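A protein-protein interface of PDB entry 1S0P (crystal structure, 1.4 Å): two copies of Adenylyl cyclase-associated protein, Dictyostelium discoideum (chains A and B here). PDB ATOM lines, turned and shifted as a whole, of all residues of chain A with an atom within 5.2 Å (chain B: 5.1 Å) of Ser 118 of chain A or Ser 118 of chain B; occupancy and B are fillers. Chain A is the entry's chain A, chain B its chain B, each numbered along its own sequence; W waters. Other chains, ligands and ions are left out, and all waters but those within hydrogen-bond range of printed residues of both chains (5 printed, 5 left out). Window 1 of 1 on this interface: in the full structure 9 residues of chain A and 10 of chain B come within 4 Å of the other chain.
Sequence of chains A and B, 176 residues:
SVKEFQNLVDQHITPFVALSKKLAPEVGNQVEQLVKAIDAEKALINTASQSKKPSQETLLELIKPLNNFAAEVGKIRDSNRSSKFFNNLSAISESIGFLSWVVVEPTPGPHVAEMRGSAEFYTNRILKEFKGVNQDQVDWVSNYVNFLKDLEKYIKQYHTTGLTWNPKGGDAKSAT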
ATOM      1  N   GLU A  94     -27.286 -14.677   8.366  1.00  0.00           N
ATOM      2  CA  GLU A  94     -27.812 -16.031   8.505  1.00  0.00           C
ATOM      3  C   GLU A  94     -28.134 -16.431   9.907  1.00  0.00           C
ATOM      4  O   GLU A  94     -28.653 -17.522  10.129  1.00  0.00           O
ATOM      5  CB  GLU A  94     -26.843 -17.047   7.821  1.00  0.00           C
ATOM      6  CG  GLU A  94     -26.496 -16.720   6.350  1.00  0.00           C
ATOM      7  CD  GLU A  94     -27.732 -16.228   5.588  1.00  0.00           C
ATOM      8  OE1 GLU A  94     -27.781 -15.110   5.066  1.00  0.00           O
ATOM      9  OE2 GLU A  94     -28.715 -17.025   5.501  1.00  0.00           O
ATOM     10  N   SER A  95     -27.956 -15.514  10.860  1.00  0.00           N
ATOM     11  CA  SER A  95     -28.251 -15.779  12.302  1.00  0.00           C
ATOM     12  C   SER A  95     -28.951 -14.594  12.841  1.00  0.00           C
ATOM     13  O   SER A  95     -28.871 -14.432  14.058  1.00  0.00           O
ATOM     14  CB  SER A  95     -26.923 -15.955  13.106  1.00  0.00           C
ATOM     15  OG  SER A  95     -26.249 -14.689  13.195  1.00  0.00           O
ATOM     16  N   GLU A 114     -29.797 -22.576  17.731  1.00  0.00           N
ATOM     17  CA  GLU A 114     -29.901 -22.929  16.297  1.00  0.00           C
ATOM     18  C   GLU A 114     -29.249 -21.853  15.483  1.00  0.00           C
ATOM     19  O   GLU A 114     -28.445 -22.099  14.549  1.00  0.00           O
ATOM     20  CB  GLU A 114     -31.360 -23.067  15.901  1.00  0.00           C
ATOM     21  CG  GLU A 114     -31.629 -23.069  14.364  1.00  0.00           C
ATOM     22  CD  GLU A 114     -31.327 -24.384  13.692  1.00  0.00           C
ATOM     23  OE1 GLU A 114     -31.186 -24.381  12.430  1.00  0.00           O
ATOM     24  OE2 GLU A 114     -31.264 -25.379  14.398  1.00  0.00           O
ATOM     25  N   MET A 115     -29.523 -20.608  15.837  1.00  0.00           N
ATOM     26  CA  MET A 115     -28.959 -19.495  15.069  1.00  0.00           C
ATOM     27  C   MET A 115     -27.497 -19.339  15.284  1.00  0.00           C
ATOM     28  O   MET A 115     -26.796 -18.944  14.300  1.00  0.00           O
ATOM     29  CB  MET A 115     -29.690 -18.196  15.459  1.00  0.00           C
ATOM     30  CG  MET A 115     -31.192 -18.254  15.190  1.00  0.00           C
ATOM     31  SD  MET A 115     -31.649 -18.800  13.478  1.00  0.00           S
ATOM     32  CE  MET A 115     -33.332 -19.492  13.807  1.00  0.00           C
ATOM     33  N   ARG A 116     -26.980 -19.637  16.471  1.00  0.00           N
ATOM     34  CA  ARG A 116     -25.542 -19.599  16.657  1.00  0.00           C
ATOM     35  C   ARG A 116     -24.851 -20.648  15.747  1.00  0.00           C
ATOM     36  O   ARG A 116     -23.779 -20.363  15.242  1.00  0.00           O
ATOM     37  CB  ARG A 116     -25.172 -19.829  18.143  1.00  0.00           C
ATOM     38  CG  ARG A 116     -23.655 -19.761  18.376  1.00  0.00           C
ATOM     39  CD  ARG A 116     -23.296 -19.604  19.824  1.00  0.00           C
ATOM     40  NE  ARG A 116     -23.361 -20.829  20.604  1.00  0.00           N
ATOM     41  CZ  ARG A 116     -24.388 -21.642  20.738  1.00  0.00           C
ATOM     42  NH1 ARG A 116     -25.546 -21.388  20.122  1.00  0.00           N
ATOM     43  NH2 ARG A 116     -24.286 -22.721  21.525  1.00  0.00           N
ATOM     44  N   GLY A 117     -25.451 -21.822  15.606  1.00  0.00           N
ATOM     45  CA  GLY A 117     -24.863 -22.853  14.741  1.00  0.00           C
ATOM     46  C   GLY A 117     -24.757 -22.237  13.322  1.00  0.00           C
ATOM     47  O   GLY A 117     -23.770 -22.477  12.613  1.00  0.00           O
ATOM     48  N   SER A 118     -25.737 -21.518  12.853  1.00  0.00           N
ATOM     49  CA  SER A 118     -25.700 -20.923  11.514  1.00  0.00           C
ATOM     50  C   SER A 118     -24.658 -19.873  11.467  1.00  0.00           C
ATOM     51  O   SER A 118     -23.884 -19.792  10.497  1.00  0.00           O
ATOM     52  CB  SER A 118     -27.004 -20.340  11.135  1.00  0.00           C
ATOM     53  OG  SER A 118     -27.993 -21.388  11.079  1.00  0.00           O
ATOM     54  N   ALA A 119     -24.488 -19.017  12.492  1.00  0.00           N
ATOM     55  CA  ALA A 119     -23.430 -18.033  12.482  1.00  0.00           C
ATOM     56  C   ALA A 119     -22.071 -18.727  12.397  1.00  0.00           C
ATOM     57  O   ALA A 119     -21.201 -18.256  11.655  1.00  0.00           O
ATOM     58  CB  ALA A 119     -23.537 -17.192  13.772  1.00  0.00           C
ATOM     59  N   GLU A 120     -21.890 -19.769  13.215  1.00  0.00           N
ATOM     60  CA  GLU A 120     -20.619 -20.459  13.293  1.00  0.00           C
ATOM     61  C   GLU A 120     -20.189 -21.100  12.016  1.00  0.00           C
ATOM     62  O   GLU A 120     -18.960 -21.252  11.786  1.00  0.00           O
ATOM     63  CB  GLU A 120     -20.625 -21.456  14.433  1.00  0.00           C
ATOM     64  CG  GLU A 120     -20.579 -20.776  15.842  1.00  0.00           C
ATOM     65  CD  GLU A 120     -20.811 -21.744  17.016  1.00  0.00           C
ATOM     66  OE1 GLU A 120     -21.213 -22.896  16.830  1.00  0.00           O
ATOM     67  OE2 GLU A 120     -20.611 -21.294  18.148  1.00  0.00           O
ATOM     68  N   PHE A 121     -21.148 -21.519  11.186  1.00  0.00           N
ATOM     69  CA  PHE A 121     -20.755 -22.093   9.886  1.00  0.00           C
ATOM     70  C   PHE A 121     -19.915 -21.050   9.174  1.00  0.00           C
ATOM     71  O   PHE A 121     -18.936 -21.409   8.478  1.00  0.00           O
ATOM     72  CB  PHE A 121     -22.015 -22.384   9.112  1.00  0.00           C
ATOM     73  CG  PHE A 121     -21.744 -23.132   7.768  1.00  0.00           C
ATOM     74  CD1 PHE A 121     -21.330 -24.479   7.767  1.00  0.00           C
ATOM     75  CD2 PHE A 121     -21.941 -22.470   6.555  1.00  0.00           C
ATOM     76  CE1 PHE A 121     -21.119 -25.142   6.544  1.00  0.00           C
ATOM     77  CE2 PHE A 121     -21.731 -23.153   5.334  1.00  0.00           C
ATOM     78  CZ  PHE A 121     -21.333 -24.449   5.332  1.00  0.00           C
ATOM     79  N   TYR A 122     -20.274 -19.759   9.248  1.00  0.00           N
ATOM     80  CA  TYR A 122     -19.457 -18.724   8.617  1.00  0.00           C
ATOM     81  C   TYR A 122     -18.316 -18.228   9.444  1.00  0.00           C
ATOM     82  O   TYR A 122     -17.193 -17.976   8.906  1.00  0.00           O
ATOM     83  CB  TYR A 122     -20.336 -17.542   8.242  1.00  0.00           C
ATOM     84  CG  TYR A 122     -21.464 -17.927   7.262  1.00  0.00           C
ATOM     85  CD1 TYR A 122     -22.746 -18.269   7.743  1.00  0.00           C
ATOM     86  CD2 TYR A 122     -21.213 -18.113   5.898  1.00  0.00           C
ATOM     87  CE1 TYR A 122     -23.744 -18.837   6.901  1.00  0.00           C
ATOM     88  CE2 TYR A 122     -22.215 -18.617   5.045  1.00  0.00           C
ATOM     89  CZ  TYR A 122     -23.445 -18.983   5.584  1.00  0.00           C
ATOM     90  OH  TYR A 122     -24.522 -19.538   4.834  1.00  0.00           O
ATOM     91  N   GLU B  94     -33.738 -19.446   4.150  1.00  0.00           N
ATOM     92  CA  GLU B  94     -32.672 -19.765   5.077  1.00  0.00           C
ATOM     93  C   GLU B  94     -31.823 -20.914   4.646  1.00  0.00           C
ATOM     94  O   GLU B  94     -30.808 -21.191   5.283  1.00  0.00           O
ATOM     95  CB  GLU B  94     -33.281 -19.942   6.496  1.00  0.00           C
ATOM     96  CG  GLU B  94     -34.108 -18.756   6.962  1.00  0.00           C
ATOM     97  CD  GLU B  94     -33.519 -17.352   6.612  1.00  0.00           C
ATOM     98  OE1 GLU B  94     -34.136 -16.570   5.860  1.00  0.00           O
ATOM     99  OE2 GLU B  94     -32.381 -17.129   7.101  1.00  0.00           O
ATOM    100  N   SER B  95     -32.150 -21.540   3.525  1.00  0.00           N
ATOM    101  CA  SER B  95     -31.363 -22.649   3.023  1.00  0.00           C
ATOM    102  C   SER B  95     -30.906 -22.434   1.585  1.00  0.00           C
ATOM    103  O   SER B  95     -30.219 -23.343   1.060  1.00  0.00           O
ATOM    104  CB  SER B  95     -32.185 -23.929   3.112  1.00  0.00           C
ATOM    105  OG  SER B  95     -33.336 -23.908   2.261  1.00  0.00           O
ATOM    106  N   GLU B 114     -25.640 -28.795   5.777  1.00  0.00           N
ATOM    107  CA  GLU B 114     -25.777 -27.707   6.735  1.00  0.00           C
ATOM    108  C   GLU B 114     -27.001 -26.888   6.328  1.00  0.00           C
ATOM    109  O   GLU B 114     -27.769 -26.483   7.155  1.00  0.00           O
ATOM    110  CB  GLU B 114     -24.579 -26.791   6.680  1.00  0.00           C
ATOM    111  CG  GLU B 114     -24.833 -25.346   7.173  1.00  0.00           C
ATOM    112  CD  GLU B 114     -24.813 -25.226   8.696  1.00  0.00           C
ATOM    113  OE1 GLU B 114     -25.226 -24.135   9.201  1.00  0.00           O
ATOM    114  OE2 GLU B 114     -24.383 -26.209   9.342  1.00  0.00           O
ATOM    115  N   MET B 115     -27.214 -26.656   5.034  1.00  0.00           N
ATOM    116  CA  MET B 115     -28.359 -25.847   4.587  1.00  0.00           C
ATOM    117  C   MET B 115     -29.632 -26.625   4.743  1.00  0.00           C
ATOM    118  O   MET B 115     -30.686 -26.015   5.057  1.00  0.00           O
ATOM    119  CB  MET B 115     -28.180 -25.469   3.126  1.00  0.00           C
ATOM    120  CG  MET B 115     -26.870 -24.675   2.876  1.00  0.00           C
ATOM    121  SD  MET B 115     -26.758 -23.161   3.990  1.00  0.00           S
ATOM    122  CE  MET B 115     -25.092 -22.693   3.844  1.00  0.00           C
ATOM    123  N   ARG B 116     -29.615 -27.922   4.604  1.00  0.00           N
ATOM    124  CA  ARG B 116     -30.790 -28.699   4.847  1.00  0.00           C
ATOM    125  C   ARG B 116     -31.179 -28.582   6.347  1.00  0.00           C
ATOM    126  O   ARG B 116     -32.382 -28.554   6.644  1.00  0.00           O
ATOM    127  CB  ARG B 116     -30.600 -30.177   4.442  1.00  0.00           C
ATOM    128  CG  ARG B 116     -31.867 -30.993   4.697  1.00  0.00           C
ATOM    129  CD  ARG B 116     -31.854 -32.410   4.111  1.00  0.00           C
ATOM    130  NE  ARG B 116     -30.620 -33.115   4.432  1.00  0.00           N
ATOM    131  CZ  ARG B 116     -30.380 -33.876   5.496  1.00  0.00           C
ATOM    132  NH1 ARG B 116     -31.290 -34.105   6.449  1.00  0.00           N
ATOM    133  NH2 ARG B 116     -29.165 -34.406   5.590  1.00  0.00           N
ATOM    134  N   GLY B 117     -30.215 -28.579   7.283  1.00  0.00           N
ATOM    135  CA  GLY B 117     -30.603 -28.444   8.688  1.00  0.00           C
ATOM    136  C   GLY B 117     -31.304 -27.117   8.839  1.00  0.00           C
ATOM    137  O   GLY B 117     -32.270 -27.055   9.666  1.00  0.00           O
ATOM    138  N   SER B 118     -30.874 -26.064   8.190  1.00  0.00           N
ATOM    139  CA  SER B 118     -31.553 -24.794   8.353  1.00  0.00           C
ATOM    140  C   SER B 118     -32.948 -24.862   7.777  1.00  0.00           C
ATOM    141  O   SER B 118     -33.883 -24.352   8.355  1.00  0.00           O
ATOM    142  CB  SER B 118     -30.788 -23.664   7.707  1.00  0.00           C
ATOM    143  OG  SER B 118     -29.536 -23.541   8.395  1.00  0.00           O
ATOM    144  N   ALA B 119     -33.170 -25.518   6.645  1.00  0.00           N
ATOM    145  CA  ALA B 119     -34.481 -25.655   6.066  1.00  0.00           C
ATOM    146  C   ALA B 119     -35.397 -26.438   7.033  1.00  0.00           C
ATOM    147  O   ALA B 119     -36.556 -26.064   7.215  1.00  0.00           O
ATOM    148  CB  ALA B 119     -34.388 -26.431   4.719  1.00  0.00           C
ATOM    149  N   GLU B 120     -34.874 -27.515   7.625  1.00  0.00           N
ATOM    150  CA  GLU B 120     -35.687 -28.370   8.483  1.00  0.00           C
ATOM    151  C   GLU B 120     -36.114 -27.661   9.765  1.00  0.00           C
ATOM    152  O   GLU B 120     -37.146 -28.038  10.317  1.00  0.00           O
ATOM    153  CB  GLU B 120     -34.962 -29.679   8.783  1.00  0.00           C
ATOM    154  CG  GLU B 120     -34.923 -30.578   7.539  1.00  0.00           C
ATOM    155  CD  GLU B 120     -34.029 -31.789   7.725  1.00  0.00           C
ATOM    156  OE1 GLU B 120     -33.185 -31.757   8.661  1.00  0.00           O
ATOM    157  OE2 GLU B 120     -34.108 -32.702   6.925  1.00  0.00           O
ATOM    158  N   PHE B 121     -35.314 -26.724  10.241  1.00  0.00           N
ATOM    159  CA  PHE B 121     -35.746 -25.997  11.416  1.00  0.00           C
ATOM    160  C   PHE B 121     -37.130 -25.400  11.150  1.00  0.00           C
ATOM    161  O   PHE B 121     -38.000 -25.354  12.023  1.00  0.00           O
ATOM    162  CB  PHE B 121     -34.704 -24.869  11.737  1.00  0.00           C
ATOM    163  CG  PHE B 121     -34.991 -24.105  12.994  1.00  0.00           C
ATOM    164  CD1 PHE B 121     -34.809 -24.715  14.246  1.00  0.00           C
ATOM    165  CD2 PHE B 121     -35.394 -22.784  12.919  1.00  0.00           C
ATOM    166  CE1 PHE B 121     -35.051 -23.953  15.446  1.00  0.00           C
ATOM    167  CE2 PHE B 121     -35.616 -22.047  14.090  1.00  0.00           C
ATOM    168  CZ  PHE B 121     -35.440 -22.640  15.322  1.00  0.00           C
ATOM    169  N   TYR B 122     -37.332 -24.921   9.913  1.00  0.00           N
ATOM    170  CA  TYR B 122     -38.633 -24.373   9.519  1.00  0.00           C
ATOM    171  C   TYR B 122     -39.612 -25.426   9.020  1.00  0.00           C
ATOM    172  O   TYR B 122     -40.802 -25.384   9.364  1.00  0.00           O
ATOM    173  CB  TYR B 122     -38.522 -23.261   8.458  1.00  0.00           C
ATOM    174  CG  TYR B 122     -37.611 -22.122   8.941  1.00  0.00           C
ATOM    175  CD1 TYR B 122     -36.245 -22.105   8.621  1.00  0.00           C
ATOM    176  CD2 TYR B 122     -38.109 -21.160   9.833  1.00  0.00           C
ATOM    177  CE1 TYR B 122     -35.347 -21.196   9.167  1.00  0.00           C
ATOM    178  CE2 TYR B 122     -37.189 -20.179  10.411  1.00  0.00           C
ATOM    179  CZ  TYR B 122     -35.855 -20.247  10.061  1.00  0.00           C
ATOM    180  OH  TYR B 122     -34.946 -19.365  10.597  1.00  0.00           O
HETATM  181  O   HOH W   1     -27.109 -22.400   8.211  1.00  0.00           O
HETATM  182  O   HOH W   2     -30.774 -18.701   8.620  1.00  0.00           O
HETATM  183  O   HOH W   3     -26.611 -20.587   6.016  1.00  0.00           O
HETATM  184  O   HOH W   4     -32.559 -19.891  10.367  1.00  0.00           O
HETATM  185  O   HOH W   5     -30.611 -22.046  10.818  1.00  0.00           O
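Water W4 lies within hydrogen-bond range of the side-chain hydroxyl (OH) of Tyr 122 of chain B and the side-chain sulfur (SD) of Met 115 of chain A.
Water W3 bridges OH of Tyr 122 of chain A (2.6 Å) and SD of Met 115 of chain B (3.3 Å).
Water W1 lies within hydrogen-bond range of OG of Ser 118 of chain B (2.7 Å), OE1 of Glu 114 of chain B (2.7 Å) and OG of Ser 118 of chain A (3.2 Å).
Water W5 lies within hydrogen-bond range of OG of Ser 118 of chain A (2.7 Å), OE1 of Glu 114 of chain A (2.9 Å) and OG of Ser 118 of chain B (3.0 Å).
Water W2 bridges the side-chain carboxylate of Glu 94 of chain B (2.7 Å) and the backbone carbonyl oxygen of Glu 94 of chain A (2.9 Å).
Among the printed residues, merely in contact across the chains: Tyr 122 of chain A with Met 115 of chain B (3.4 Å), Met 115 of chain A with Phe 121 of chain B (3.4 Å), Glu 114 of chain A with Phe 121 of chain B (3.5 Å), Met 115 of chain A with Tyr 122 of chain B (3.6 Å), Phe 121 of chain A with Glu 114 of chain B (3.7 Å), Phe 121 of chain A with Met 115 of chain B (3.7 Å), Ser 118 of chain A with Ser 118 of chain B (3.8 Å), Ser 118 of chain A with Glu 114 of chain B (3.99 Å) and Glu 114 of chain A with Gly 117 of chain B (3.996 Å).
Of the printed residues of chain B, Met 115 of chain A touches Phe 121 and Tyr 122.
Of the printed residues of chain B, Ser 118 of chain A touches Glu 114 (3.99 Å) and Ser 118 (3.8 Å).
Of the printed residues of chain A, Glu 114 of chain B touches Ser 118 (3.99 Å) and Phe 121 (3.7 Å).
Of the printed residues of chain A, Met 115 of chain B touches Phe 121 and Tyr 122.
Ser 118 of chain B touches just one residue of chain A: Ser 118.
Printed residues of chain A within 4 Å of Phe 121 of chain B: Glu 114 and Met 115.
The nearest residue of chain A that does not touch Ser 118 of chain B is Glu 114 of chain A (4.1 Å).
Glu 114 of chain A touches Phe 121 of chain B, and with the chains exchanged Phe 121 of chain A touches Glu 114 of chain B.
Met 115 of chain A touches Phe 121 of chain B, and with the chains exchanged Phe 121 of chain A touches Met 115 of chain B.
Ser 118 of chain A touches Glu 114 of chain B, but with the chains exchanged Glu 114 of chain A does not touch Ser 118 of chain B (4.1 Å).
Ser 118 of chain A touches its own counterpart, Ser 118 of chain B.
Positions printed for both chains: 94, 95, 114, 115, 116, 117, 118, 119, 120, 121 and 122.
Of the 9 pairs that touch across the chains among the printed residues, 7 have their exchanged pair printed and touching as well.
Of the 11 printed residues of chain B, 6 touch a printed residue of chain A.
Of the 11 printed residues of chain A, 5 touch a printed residue of chain B.
Hydrophobic or aromatic side chains of chain A that line the printed part of chain B: Met 115, Phe 121 and Tyr 122.
Among the printed residues, no Asp or Glu carboxylate lies within 4 Å of a Lys or Arg side-chain nitrogen of the other chain.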
